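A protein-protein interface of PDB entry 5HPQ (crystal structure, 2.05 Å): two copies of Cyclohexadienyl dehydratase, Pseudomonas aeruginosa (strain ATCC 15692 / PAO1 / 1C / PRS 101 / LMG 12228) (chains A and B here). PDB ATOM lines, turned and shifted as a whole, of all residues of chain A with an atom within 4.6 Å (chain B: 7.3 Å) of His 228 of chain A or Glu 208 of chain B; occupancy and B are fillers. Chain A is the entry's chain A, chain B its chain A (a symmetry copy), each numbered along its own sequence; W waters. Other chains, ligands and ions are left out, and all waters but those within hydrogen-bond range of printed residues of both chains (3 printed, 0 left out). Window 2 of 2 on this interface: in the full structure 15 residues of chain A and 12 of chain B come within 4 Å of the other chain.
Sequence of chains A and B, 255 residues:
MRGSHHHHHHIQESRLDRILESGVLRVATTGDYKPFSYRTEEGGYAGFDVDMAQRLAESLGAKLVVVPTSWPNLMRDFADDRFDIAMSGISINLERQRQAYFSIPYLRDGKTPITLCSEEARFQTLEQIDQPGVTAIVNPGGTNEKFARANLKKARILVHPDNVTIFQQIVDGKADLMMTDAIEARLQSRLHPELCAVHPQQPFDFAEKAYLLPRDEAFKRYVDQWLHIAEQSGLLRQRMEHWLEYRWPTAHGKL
OE1 of Gln 232 of chain A lies within hydrogen-bond range of NH1 of Arg 108 of chain B (3.1 Å).
NE2 of His 228 of chain A sits at hydrogen-bond distance from OE2 of Glu 208 of chain B, 2.7 Å away.
The backbone NH (N) of Ile 92 of chain B sits at hydrogen-bond distance from the backbone carbonyl oxygen (O) of Glu 208 of chain B (2.7 Å).
Among the printed residues, merely in contact across the chains: Gln 232 of chain A with Phe 206 of chain B and Gln 225 of chain A with Ile 92 of chain B.
Of chain B, only Glu 208 comes within 4 Å of His 228 of chain A.
Of chain A, only His 228 (2.7 Å) comes within 4 Å of Glu 208 of chain B.
Of the printed residues of chain B, Gln 225 of chain A touches Ile 92.
Of the printed residues of chain A, Phe 206 of chain B touches Gln 232.
Printed residues of chain A within 4 Å of Arg 108 of chain B: Gln 232 (3.1 Å).
Printed residues of chain A within 4 Å of Ile 92 of chain B: Gln 225.
Of the printed residues of chain B, Gln 232 of chain A touches Arg 108 and Phe 206.
Tyr 106 of chain B touches none of the printed residues of chain A.
The nearest residue of chain B that does not touch His 228 of chain A is Phe 206 of chain B (4.4 Å).
The nearest residue of chain A that does not touch Glu 208 of chain B is Gln 225 of chain A (4.2 Å).
The nearest printed residue of chain A that does not touch Arg 108 of chain B is Glu 231 of chain A (7.0 Å).
Hydrophobic or aromatic side chains of chain B that line the printed part of chain A: Ile 92 and Phe 206.
Of the 10 printed residues of chain A, 3 touch a printed residue of chain B.
Printed residues of chain A that touch a printed residue of chain B: Gln 225, His 228 and Gln 232.
Hydrophobic or aromatic side chains of chain A within 4 Å of the printed part of chain B: His 228.
Along chain A the printed residues that touch a printed residue of chain B span positions 225 to 232.
Among the printed residues, 4 pairs touch across the chains.
Position printed for both chains: 104.
Of the 4 pairs that touch across the chains among the printed residues, none has its exchanged pair printed and touching as well.
Water W3 lies within hydrogen-bond range of OE1 of Glu 208 of chain B (2.6 Å) and OE1 of Gln 225 of chain A (3.4 Å).
Water W1 bridges the side-chain carboxylate of Glu 208 of chain B (2.7 Å) and the side-chain amide oxygen of Gln 225 of chain A (2.8 Å).
Water W2 bridges NE2 of Gln 225 of chain A and O of Ser 103 of chain B.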
ATOM      1  N   ILE A 104      -2.420 -10.931  28.215  1.00  0.00           N
ATOM      2  CA  ILE A 104      -1.241 -11.300  27.406  1.00  0.00           C
ATOM      3  C   ILE A 104      -0.348 -10.006  27.196  1.00  0.00           C
ATOM      4  O   ILE A 104      -0.828  -8.846  27.305  1.00  0.00           O
ATOM      5  CB  ILE A 104      -1.572 -11.999  26.055  1.00  0.00           C
ATOM      6  CG1 ILE A 104      -2.445 -11.093  25.163  1.00  0.00           C
ATOM      7  CG2 ILE A 104      -2.212 -13.412  26.288  1.00  0.00           C
ATOM      8  CD1 ILE A 104      -2.647 -11.727  23.747  1.00  0.00           C
ATOM      9  N   ASP A 224      -7.673 -10.217  26.270  1.00  0.00           N
ATOM     10  CA  ASP A 224      -6.664 -10.950  25.519  1.00  0.00           C
ATOM     11  C   ASP A 224      -7.098 -11.176  24.082  1.00  0.00           C
ATOM     12  O   ASP A 224      -6.291 -11.080  23.203  1.00  0.00           O
ATOM     13  CB  ASP A 224      -6.412 -12.316  26.137  1.00  0.00           C
ATOM     14  CG  ASP A 224      -5.667 -12.235  27.476  1.00  0.00           C
ATOM     15  OD1 ASP A 224      -5.090 -11.128  27.799  1.00  0.00           O
ATOM     16  OD2 ASP A 224      -5.602 -13.310  28.159  1.00  0.00           O
ATOM     17  N   GLN A 225      -8.357 -11.534  23.858  1.00  0.00           N
ATOM     18  CA  GLN A 225      -8.799 -11.681  22.486  1.00  0.00           C
ATOM     19  C   GLN A 225      -8.645 -10.362  21.692  1.00  0.00           C
ATOM     20  O   GLN A 225      -8.155 -10.389  20.537  1.00  0.00           O
ATOM     21  CB  GLN A 225     -10.229 -12.198  22.381  1.00  0.00           C
ATOM     22  CG  GLN A 225     -10.526 -12.885  21.075  1.00  0.00           C
ATOM     23  CD  GLN A 225      -9.749 -14.179  20.950  1.00  0.00           C
ATOM     24  OE1 GLN A 225      -8.805 -14.255  20.225  1.00  0.00           O
ATOM     25  NE2 GLN A 225     -10.205 -15.208  21.598  1.00  0.00           N
ATOM     26  N   TRP A 226      -9.032  -9.248  22.310  1.00  0.00           N
ATOM     27  CA  TRP A 226      -8.932  -7.938  21.672  1.00  0.00           C
ATOM     28  C   TRP A 226      -7.454  -7.597  21.389  1.00  0.00           C
ATOM     29  O   TRP A 226      -7.111  -7.049  20.325  1.00  0.00           O
ATOM     30  CB  TRP A 226      -9.578  -6.884  22.548  1.00  0.00           C
ATOM     31  CG  TRP A 226      -9.123  -5.473  22.285  1.00  0.00           C
ATOM     32  CD1 TRP A 226      -9.530  -4.663  21.292  1.00  0.00           C
ATOM     33  CD2 TRP A 226      -8.121  -4.729  23.026  1.00  0.00           C
ATOM     34  NE1 TRP A 226      -8.858  -3.469  21.362  1.00  0.00           N
ATOM     35  CE2 TRP A 226      -8.006  -3.477  22.421  1.00  0.00           C
ATOM     36  CE3 TRP A 226      -7.327  -5.011  24.139  1.00  0.00           C
ATOM     37  CZ2 TRP A 226      -7.117  -2.513  22.887  1.00  0.00           C
ATOM     38  CZ3 TRP A 226      -6.481  -4.064  24.609  1.00  0.00           C
ATOM     39  CH2 TRP A 226      -6.387  -2.830  24.010  1.00  0.00           C
ATOM     40  N   LEU A 227      -6.583  -7.912  22.348  1.00  0.00           N
ATOM     41  CA  LEU A 227      -5.171  -7.550  22.196  1.00  0.00           C
ATOM     42  C   LEU A 227      -4.481  -8.423  21.171  1.00  0.00           C
ATOM     43  O   LEU A 227      -3.572  -7.944  20.437  1.00  0.00           O
ATOM     44  CB  LEU A 227      -4.447  -7.706  23.530  1.00  0.00           C
ATOM     45  CG  LEU A 227      -3.097  -7.010  23.786  1.00  0.00           C
ATOM     46  CD1 LEU A 227      -3.139  -5.579  23.288  1.00  0.00           C
ATOM     47  CD2 LEU A 227      -2.793  -7.137  25.278  1.00  0.00           C
ATOM     48  N   HIS A 228      -4.842  -9.719  21.152  1.00  0.00           N
ATOM     49  CA  HIS A 228      -4.236 -10.608  20.188  1.00  0.00           C
ATOM     50  C   HIS A 228      -4.557 -10.132  18.747  1.00  0.00           C
ATOM     51  O   HIS A 228      -3.728 -10.201  17.883  1.00  0.00           O
ATOM     52  CB  HIS A 228      -4.786 -11.988  20.408  1.00  0.00           C
ATOM     53  CG  HIS A 228      -4.397 -12.999  19.380  1.00  0.00           C
ATOM     54  ND1 HIS A 228      -3.109 -13.477  19.254  1.00  0.00           N
ATOM     55  CD2 HIS A 228      -5.151 -13.721  18.520  1.00  0.00           C
ATOM     56  CE1 HIS A 228      -3.085 -14.454  18.356  1.00  0.00           C
ATOM     57  NE2 HIS A 228      -4.314 -14.616  17.882  1.00  0.00           N
ATOM     58  N   ILE A 229      -5.780  -9.665  18.515  1.00  0.00           N
ATOM     59  CA  ILE A 229      -6.180  -9.198  17.185  1.00  0.00           C
ATOM     60  C   ILE A 229      -5.473  -7.870  16.861  1.00  0.00           C
ATOM     61  O   ILE A 229      -5.026  -7.681  15.744  1.00  0.00           O
ATOM     62  CB  ILE A 229      -7.714  -9.000  17.087  1.00  0.00           C
ATOM     63  CG1 ILE A 229      -8.418 -10.352  17.055  1.00  0.00           C
ATOM     64  CG2 ILE A 229      -8.107  -8.206  15.824  1.00  0.00           C
ATOM     65  CD1 ILE A 229      -9.924 -10.281  17.294  1.00  0.00           C
ATOM     66  N   ALA A 230      -5.435  -6.945  17.825  1.00  0.00           N
ATOM     67  CA  ALA A 230      -4.650  -5.700  17.666  1.00  0.00           C
ATOM     68  C   ALA A 230      -3.188  -5.981  17.236  1.00  0.00           C
ATOM     69  O   ALA A 230      -2.686  -5.347  16.322  1.00  0.00           O
ATOM     70  CB  ALA A 230      -4.697  -4.859  18.926  1.00  0.00           C
ATOM     71  N   GLU A 231      -2.583  -6.989  17.849  1.00  0.00           N
ATOM     72  CA  GLU A 231      -1.223  -7.443  17.567  1.00  0.00           C
ATOM     73  C   GLU A 231      -1.068  -8.101  16.217  1.00  0.00           C
ATOM     74  O   GLU A 231      -0.229  -7.655  15.410  1.00  0.00           O
ATOM     75  CB  GLU A 231      -0.739  -8.409  18.663  1.00  0.00           C
ATOM     76  CG  GLU A 231       0.538  -9.205  18.351  1.00  0.00           C
ATOM     77  CD  GLU A 231       1.175  -9.786  19.598  1.00  0.00           C
ATOM     78  OE1 GLU A 231       0.701 -10.842  20.087  1.00  0.00           O
ATOM     79  OE2 GLU A 231       2.126  -9.166  20.120  1.00  0.00           O
ATOM     80  N   GLN A 232      -1.849  -9.153  15.968  1.00  0.00           N
ATOM     81  CA  GLN A 232      -1.739  -9.901  14.722  1.00  0.00           C
ATOM     82  C   GLN A 232      -2.181  -9.066  13.544  1.00  0.00           C
ATOM     83  O   GLN A 232      -1.708  -9.264  12.448  1.00  0.00           O
ATOM     84  CB  GLN A 232      -2.503 -11.224  14.766  1.00  0.00           C
ATOM     85  CG  GLN A 232      -2.005 -12.142  15.857  1.00  0.00           C
ATOM     86  CD  GLN A 232      -0.541 -12.505  15.648  1.00  0.00           C
ATOM     87  OE1 GLN A 232      -0.134 -12.815  14.533  1.00  0.00           O
ATOM     88  NE2 GLN A 232       0.264 -12.423  16.706  1.00  0.00           N
ATOM     89  N   GLY B  89     -16.433 -23.838  11.232  1.00  0.00           N
ATOM     90  CA  GLY B  89     -15.739 -22.733  10.546  1.00  0.00           C
ATOM     91  C   GLY B  89     -16.074 -21.374  11.085  1.00  0.00           C
ATOM     92  O   GLY B  89     -16.189 -20.407  10.340  1.00  0.00           O
ATOM     93  N   ILE B  90     -16.154 -21.299  12.411  1.00  0.00           N
ATOM     94  CA  ILE B  90     -16.537 -20.072  13.076  1.00  0.00           C
ATOM     95  C   ILE B  90     -15.339 -19.185  13.279  1.00  0.00           C
ATOM     96  O   ILE B  90     -14.349 -19.586  13.903  1.00  0.00           O
ATOM     97  CB  ILE B  90     -17.221 -20.393  14.436  1.00  0.00           C
ATOM     98  CG1 ILE B  90     -18.480 -21.248  14.238  1.00  0.00           C
ATOM     99  CG2 ILE B  90     -17.624 -19.122  15.121  1.00  0.00           C
ATOM    100  CD1 ILE B  90     -18.747 -22.142  15.407  1.00  0.00           C
ATOM    101  N   SER B  91     -15.443 -17.957  12.802  1.00  0.00           N
ATOM    102  CA  SER B  91     -14.439 -16.913  13.077  1.00  0.00           C
ATOM    103  C   SER B  91     -14.520 -16.399  14.511  1.00  0.00           C
ATOM    104  O   SER B  91     -15.619 -16.216  15.060  1.00  0.00           O
ATOM    105  CB  SER B  91     -14.607 -15.751  12.102  1.00  0.00           C
ATOM    106  OG  SER B  91     -14.231 -16.162  10.784  1.00  0.00           O
ATOM    107  N   ILE B  92     -13.357 -16.108  15.094  1.00  0.00           N
ATOM    108  CA  ILE B  92     -13.301 -15.353  16.293  1.00  0.00           C
ATOM    109  C   ILE B  92     -13.713 -13.901  16.032  1.00  0.00           C
ATOM    110  O   ILE B  92     -13.220 -13.306  15.109  1.00  0.00           O
ATOM    111  CB  ILE B  92     -11.868 -15.361  16.878  1.00  0.00           C
ATOM    112  CG1 ILE B  92     -11.578 -16.772  17.470  1.00  0.00           C
ATOM    113  CG2 ILE B  92     -11.746 -14.310  17.978  1.00  0.00           C
ATOM    114  CD1 ILE B  92     -10.249 -16.966  18.221  1.00  0.00           C
ATOM    115  N   ASN B  93     -14.631 -13.319  16.815  1.00  0.00           N
ATOM    116  CA  ASN B  93     -14.715 -11.847  16.799  1.00  0.00           C
ATOM    117  C   ASN B  93     -15.128 -11.371  18.146  1.00  0.00           C
ATOM    118  O   ASN B  93     -15.611 -12.193  18.947  1.00  0.00           O
ATOM    119  CB  ASN B  93     -15.566 -11.256  15.642  1.00  0.00           C
ATOM    120  CG  ASN B  93     -17.056 -11.503  15.794  1.00  0.00           C
ATOM    121  OD1 ASN B  93     -17.519 -12.034  16.795  1.00  0.00           O
ATOM    122  ND2 ASN B  93     -17.818 -11.086  14.787  1.00  0.00           N
ATOM    123  N   ARG B  96     -18.835 -11.808  19.449  1.00  0.00           N
ATOM    124  CA  ARG B  96     -19.102 -13.166  19.914  1.00  0.00           C
ATOM    125  C   ARG B  96     -18.434 -13.376  21.276  1.00  0.00           C
ATOM    126  O   ARG B  96     -19.025 -14.014  22.199  1.00  0.00           O
ATOM    127  CB  ARG B  96     -18.622 -14.201  18.905  1.00  0.00           C
ATOM    128  CG  ARG B  96     -19.669 -14.511  17.873  1.00  0.00           C
ATOM    129  CD  ARG B  96     -19.052 -15.114  16.622  1.00  0.00           C
ATOM    130  NE  ARG B  96     -20.025 -15.160  15.533  1.00  0.00           N
ATOM    131  CZ  ARG B  96     -19.706 -15.499  14.287  1.00  0.00           C
ATOM    132  NH1 ARG B  96     -18.438 -15.866  14.010  1.00  0.00           N
ATOM    133  NH2 ARG B  96     -20.667 -15.539  13.333  1.00  0.00           N
ATOM    134  N   PHE B 102     -13.870 -18.645  23.096  1.00  0.00           N
ATOM    135  CA  PHE B 102     -13.350 -19.433  22.008  1.00  0.00           C
ATOM    136  C   PHE B 102     -12.232 -20.311  22.510  1.00  0.00           C
ATOM    137  O   PHE B 102     -11.404 -19.871  23.341  1.00  0.00           O
ATOM    138  CB  PHE B 102     -12.785 -18.529  20.894  1.00  0.00           C
ATOM    139  CG  PHE B 102     -13.833 -17.813  20.139  1.00  0.00           C
ATOM    140  CD1 PHE B 102     -14.503 -18.447  19.122  1.00  0.00           C
ATOM    141  CD2 PHE B 102     -14.210 -16.529  20.484  1.00  0.00           C
ATOM    142  CE1 PHE B 102     -15.498 -17.792  18.399  1.00  0.00           C
ATOM    143  CE2 PHE B 102     -15.214 -15.876  19.779  1.00  0.00           C
ATOM    144  CZ  PHE B 102     -15.856 -16.505  18.762  1.00  0.00           C
ATOM    145  N   SER B 103     -12.111 -21.465  21.853  1.00  0.00           N
ATOM    146  CA  SER B 103     -10.924 -22.267  21.963  1.00  0.00           C
ATOM    147  C   SER B 103      -9.677 -21.490  21.470  1.00  0.00           C
ATOM    148  O   SER B 103      -9.813 -20.448  20.806  1.00  0.00           O
ATOM    149  CB  SER B 103     -11.043 -23.554  21.117  1.00  0.00           C
ATOM    150  OG  SER B 103     -10.941 -23.325  19.674  1.00  0.00           O
ATOM    151  N   ILE B 104      -8.481 -22.052  21.702  1.00  0.00           N
ATOM    152  CA  ILE B 104      -7.336 -21.605  20.885  1.00  0.00           C
ATOM    153  C   ILE B 104      -7.696 -21.811  19.355  1.00  0.00           C
ATOM    154  O   ILE B 104      -8.582 -22.628  18.987  1.00  0.00           O
ATOM    155  CB  ILE B 104      -5.976 -22.265  21.253  1.00  0.00           C
ATOM    156  CG1 ILE B 104      -6.046 -23.799  21.098  1.00  0.00           C
ATOM    157  CG2 ILE B 104      -5.497 -21.827  22.681  1.00  0.00           C
ATOM    158  CD1 ILE B 104      -4.641 -24.450  21.315  1.00  0.00           C
ATOM    159  N   PRO B 105      -7.038 -21.046  18.475  1.00  0.00           N
ATOM    160  CA  PRO B 105      -7.375 -20.990  17.032  1.00  0.00           C
ATOM    161  C   PRO B 105      -6.769 -22.139  16.290  1.00  0.00           C
ATOM    162  O   PRO B 105      -5.741 -22.668  16.722  1.00  0.00           O
ATOM    163  CB  PRO B 105      -6.806 -19.678  16.587  1.00  0.00           C
ATOM    164  CG  PRO B 105      -5.808 -19.304  17.620  1.00  0.00           C
ATOM    165  CD  PRO B 105      -6.299 -19.835  18.903  1.00  0.00           C
ATOM    166  N   TYR B 106      -7.470 -22.639  15.294  1.00  0.00           N
ATOM    167  CA  TYR B 106      -6.942 -23.751  14.498  1.00  0.00           C
ATOM    168  C   TYR B 106      -6.621 -23.278  13.069  1.00  0.00           C
ATOM    169  O   TYR B 106      -6.110 -24.047  12.265  1.00  0.00           O
ATOM    170  CB  TYR B 106      -7.850 -24.956  14.446  1.00  0.00           C
ATOM    171  CG  TYR B 106      -9.323 -24.744  14.010  1.00  0.00           C
ATOM    172  CD1 TYR B 106     -10.300 -24.361  14.928  1.00  0.00           C
ATOM    173  CD2 TYR B 106      -9.735 -24.980  12.678  1.00  0.00           C
ATOM    174  CE1 TYR B 106     -11.627 -24.180  14.531  1.00  0.00           C
ATOM    175  CE2 TYR B 106     -11.050 -24.840  12.271  1.00  0.00           C
ATOM    176  CZ  TYR B 106     -11.986 -24.450  13.196  1.00  0.00           C
ATOM    177  OH  TYR B 106     -13.261 -24.306  12.816  1.00  0.00           O
ATOM    178  N   LEU B 107      -6.952 -22.046  12.747  1.00  0.00           N
ATOM    179  CA  LEU B 107      -6.758 -21.561  11.397  1.00  0.00           C
ATOM    180  C   LEU B 107      -6.665 -20.053  11.419  1.00  0.00           C
ATOM    181  O   LEU B 107      -7.358 -19.392  12.164  1.00  0.00           O
ATOM    182  CB  LEU B 107      -7.914 -22.001  10.488  1.00  0.00           C
ATOM    183  CG  LEU B 107      -7.567 -22.022   8.982  1.00  0.00           C
ATOM    184  CD1 LEU B 107      -6.893 -23.337   8.605  1.00  0.00           C
ATOM    185  CD2 LEU B 107      -8.785 -21.811   8.055  1.00  0.00           C
ATOM    186  N   ARG B 108      -5.759 -19.513  10.629  1.00  0.00           N
ATOM    187  CA  ARG B 108      -5.689 -18.109  10.415  1.00  0.00           C
ATOM    188  C   ARG B 108      -6.190 -17.809   8.973  1.00  0.00           C
ATOM    189  O   ARG B 108      -5.902 -18.556   8.042  1.00  0.00           O
ATOM    190  CB  ARG B 108      -4.254 -17.657  10.596  1.00  0.00           C
ATOM    191  CG  ARG B 108      -4.129 -16.165  10.560  1.00  0.00           C
ATOM    192  CD  ARG B 108      -2.687 -15.727  10.827  1.00  0.00           C
ATOM    193  NE  ARG B 108      -2.440 -14.493  10.093  1.00  0.00           N
ATOM    194  CZ  ARG B 108      -1.664 -13.496  10.495  1.00  0.00           C
ATOM    195  NH1 ARG B 108      -1.023 -13.540  11.666  1.00  0.00           N
ATOM    196  NH2 ARG B 108      -1.547 -12.430   9.707  1.00  0.00           N
ATOM    197  N   ASP B 109      -6.923 -16.716   8.810  1.00  0.00           N
ATOM    198  CA  ASP B 109      -7.551 -16.368   7.524  1.00  0.00           C
ATOM    199  C   ASP B 109      -7.867 -14.854   7.461  1.00  0.00           C
ATOM    200  O   ASP B 109      -7.149 -14.028   8.015  1.00  0.00           O
ATOM    201  CB  ASP B 109      -8.808 -17.216   7.297  1.00  0.00           C
ATOM    202  CG  ASP B 109      -9.001 -17.622   5.807  1.00  0.00           C
ATOM    203  OD1 ASP B 109      -8.271 -17.144   4.916  1.00  0.00           O
ATOM    204  OD2 ASP B 109      -9.872 -18.452   5.515  1.00  0.00           O
ATOM    205  N   GLY B 110      -8.910 -14.507   6.736  1.00  0.00           N
ATOM    206  CA  GLY B 110      -9.223 -13.135   6.423  1.00  0.00           C
ATOM    207  C   GLY B 110     -10.186 -13.091   5.263  1.00  0.00           C
ATOM    208  O   GLY B 110     -10.244 -14.005   4.452  1.00  0.00           O
ATOM    209  N   ASP B 181     -14.293 -15.654   3.752  1.00  0.00           N
ATOM    210  CA  ASP B 181     -12.999 -16.169   4.149  1.00  0.00           C
ATOM    211  C   ASP B 181     -12.260 -16.715   2.926  1.00  0.00           C
ATOM    212  O   ASP B 181     -12.840 -17.459   2.138  1.00  0.00           O
ATOM    213  CB  ASP B 181     -13.143 -17.313   5.150  1.00  0.00           C
ATOM    214  CG  ASP B 181     -13.988 -16.960   6.328  1.00  0.00           C
ATOM    215  OD1 ASP B 181     -13.860 -15.850   6.864  1.00  0.00           O
ATOM    216  OD2 ASP B 181     -14.790 -17.835   6.716  1.00  0.00           O
ATOM    217  N   PHE B 206      -7.651  -9.570   9.173  1.00  0.00           N
ATOM    218  CA  PHE B 206      -7.099 -10.704   9.927  1.00  0.00           C
ATOM    219  C   PHE B 206      -8.267 -11.321  10.716  1.00  0.00           C
ATOM    220  O   PHE B 206      -9.047 -10.599  11.389  1.00  0.00           O
ATOM    221  CB  PHE B 206      -6.011 -10.243  10.883  1.00  0.00           C
ATOM    222  CG  PHE B 206      -5.649 -11.293  11.918  1.00  0.00           C
ATOM    223  CD1 PHE B 206      -4.739 -12.298  11.622  1.00  0.00           C
ATOM    224  CD2 PHE B 206      -6.260 -11.293  13.156  1.00  0.00           C
ATOM    225  CE1 PHE B 206      -4.432 -13.267  12.572  1.00  0.00           C
ATOM    226  CE2 PHE B 206      -5.976 -12.265  14.107  1.00  0.00           C
ATOM    227  CZ  PHE B 206      -5.065 -13.258  13.807  1.00  0.00           C
ATOM    228  N   ALA B 207      -8.424 -12.639  10.610  1.00  0.00           N
ATOM    229  CA  ALA B 207      -9.300 -13.387  11.553  1.00  0.00           C
ATOM    230  C   ALA B 207      -8.900 -14.832  11.711  1.00  0.00           C
ATOM    231  O   ALA B 207      -8.259 -15.424  10.813  1.00  0.00           O
ATOM    232  CB  ALA B 207     -10.744 -13.294  11.126  1.00  0.00           C
ATOM    233  N   GLU B 208      -9.282 -15.403  12.858  1.00  0.00           N
ATOM    234  CA  GLU B 208      -9.009 -16.794  13.169  1.00  0.00           C
ATOM    235  C   GLU B 208     -10.308 -17.597  13.261  1.00  0.00           C
ATOM    236  O   GLU B 208     -11.331 -17.022  13.573  1.00  0.00           O
ATOM    237  CB  GLU B 208      -8.241 -16.855  14.485  1.00  0.00           C
ATOM    238  CG  GLU B 208      -6.843 -16.264  14.400  1.00  0.00           C
ATOM    239  CD  GLU B 208      -6.191 -16.072  15.750  1.00  0.00           C
ATOM    240  OE1 GLU B 208      -6.864 -15.683  16.757  1.00  0.00           O
ATOM    241  OE2 GLU B 208      -4.978 -16.237  15.795  1.00  0.00           O
ATOM    242  N   LYS B 209     -10.247 -18.870  12.908  1.00  0.00           N
ATOM    243  CA  LYS B 209     -11.277 -19.875  13.252  1.00  0.00           C
ATOM    244  C   LYS B 209     -10.930 -20.559  14.548  1.00  0.00           C
ATOM    245  O   LYS B 209      -9.742 -20.839  14.822  1.00  0.00           O
ATOM    246  CB  LYS B 209     -11.366 -20.926  12.161  1.00  0.00           C
ATOM    247  CG  LYS B 209     -11.585 -20.362  10.705  1.00  0.00           C
ATOM    248  CD  LYS B 209     -12.814 -19.550  10.652  1.00  0.00           C
ATOM    249  CE  LYS B 209     -13.309 -19.268   9.198  1.00  0.00           C
ATOM    250  NZ  LYS B 209     -14.348 -18.255   9.479  1.00  0.00           N
ATOM    251  N   ALA B 210     -11.962 -20.797  15.344  1.00  0.00           N
ATOM    252  CA  ALA B 210     -11.854 -21.426  16.621  1.00  0.00           C
ATOM    253  C   ALA B 210     -13.227 -22.018  16.940  1.00  0.00           C
ATOM    254  O   ALA B 210     -14.240 -21.842  16.196  1.00  0.00           O
ATOM    255  CB  ALA B 210     -11.434 -20.445  17.692  1.00  0.00           C
HETATM  256  O   HOH W   1      -7.081 -16.273  19.384  1.00  0.00           O
HETATM  257  O   HOH W   2      -9.104 -17.791  21.537  1.00  0.00           O
HETATM  258  O   HOH W   3      -8.552 -13.741  16.877  1.00  0.00           O
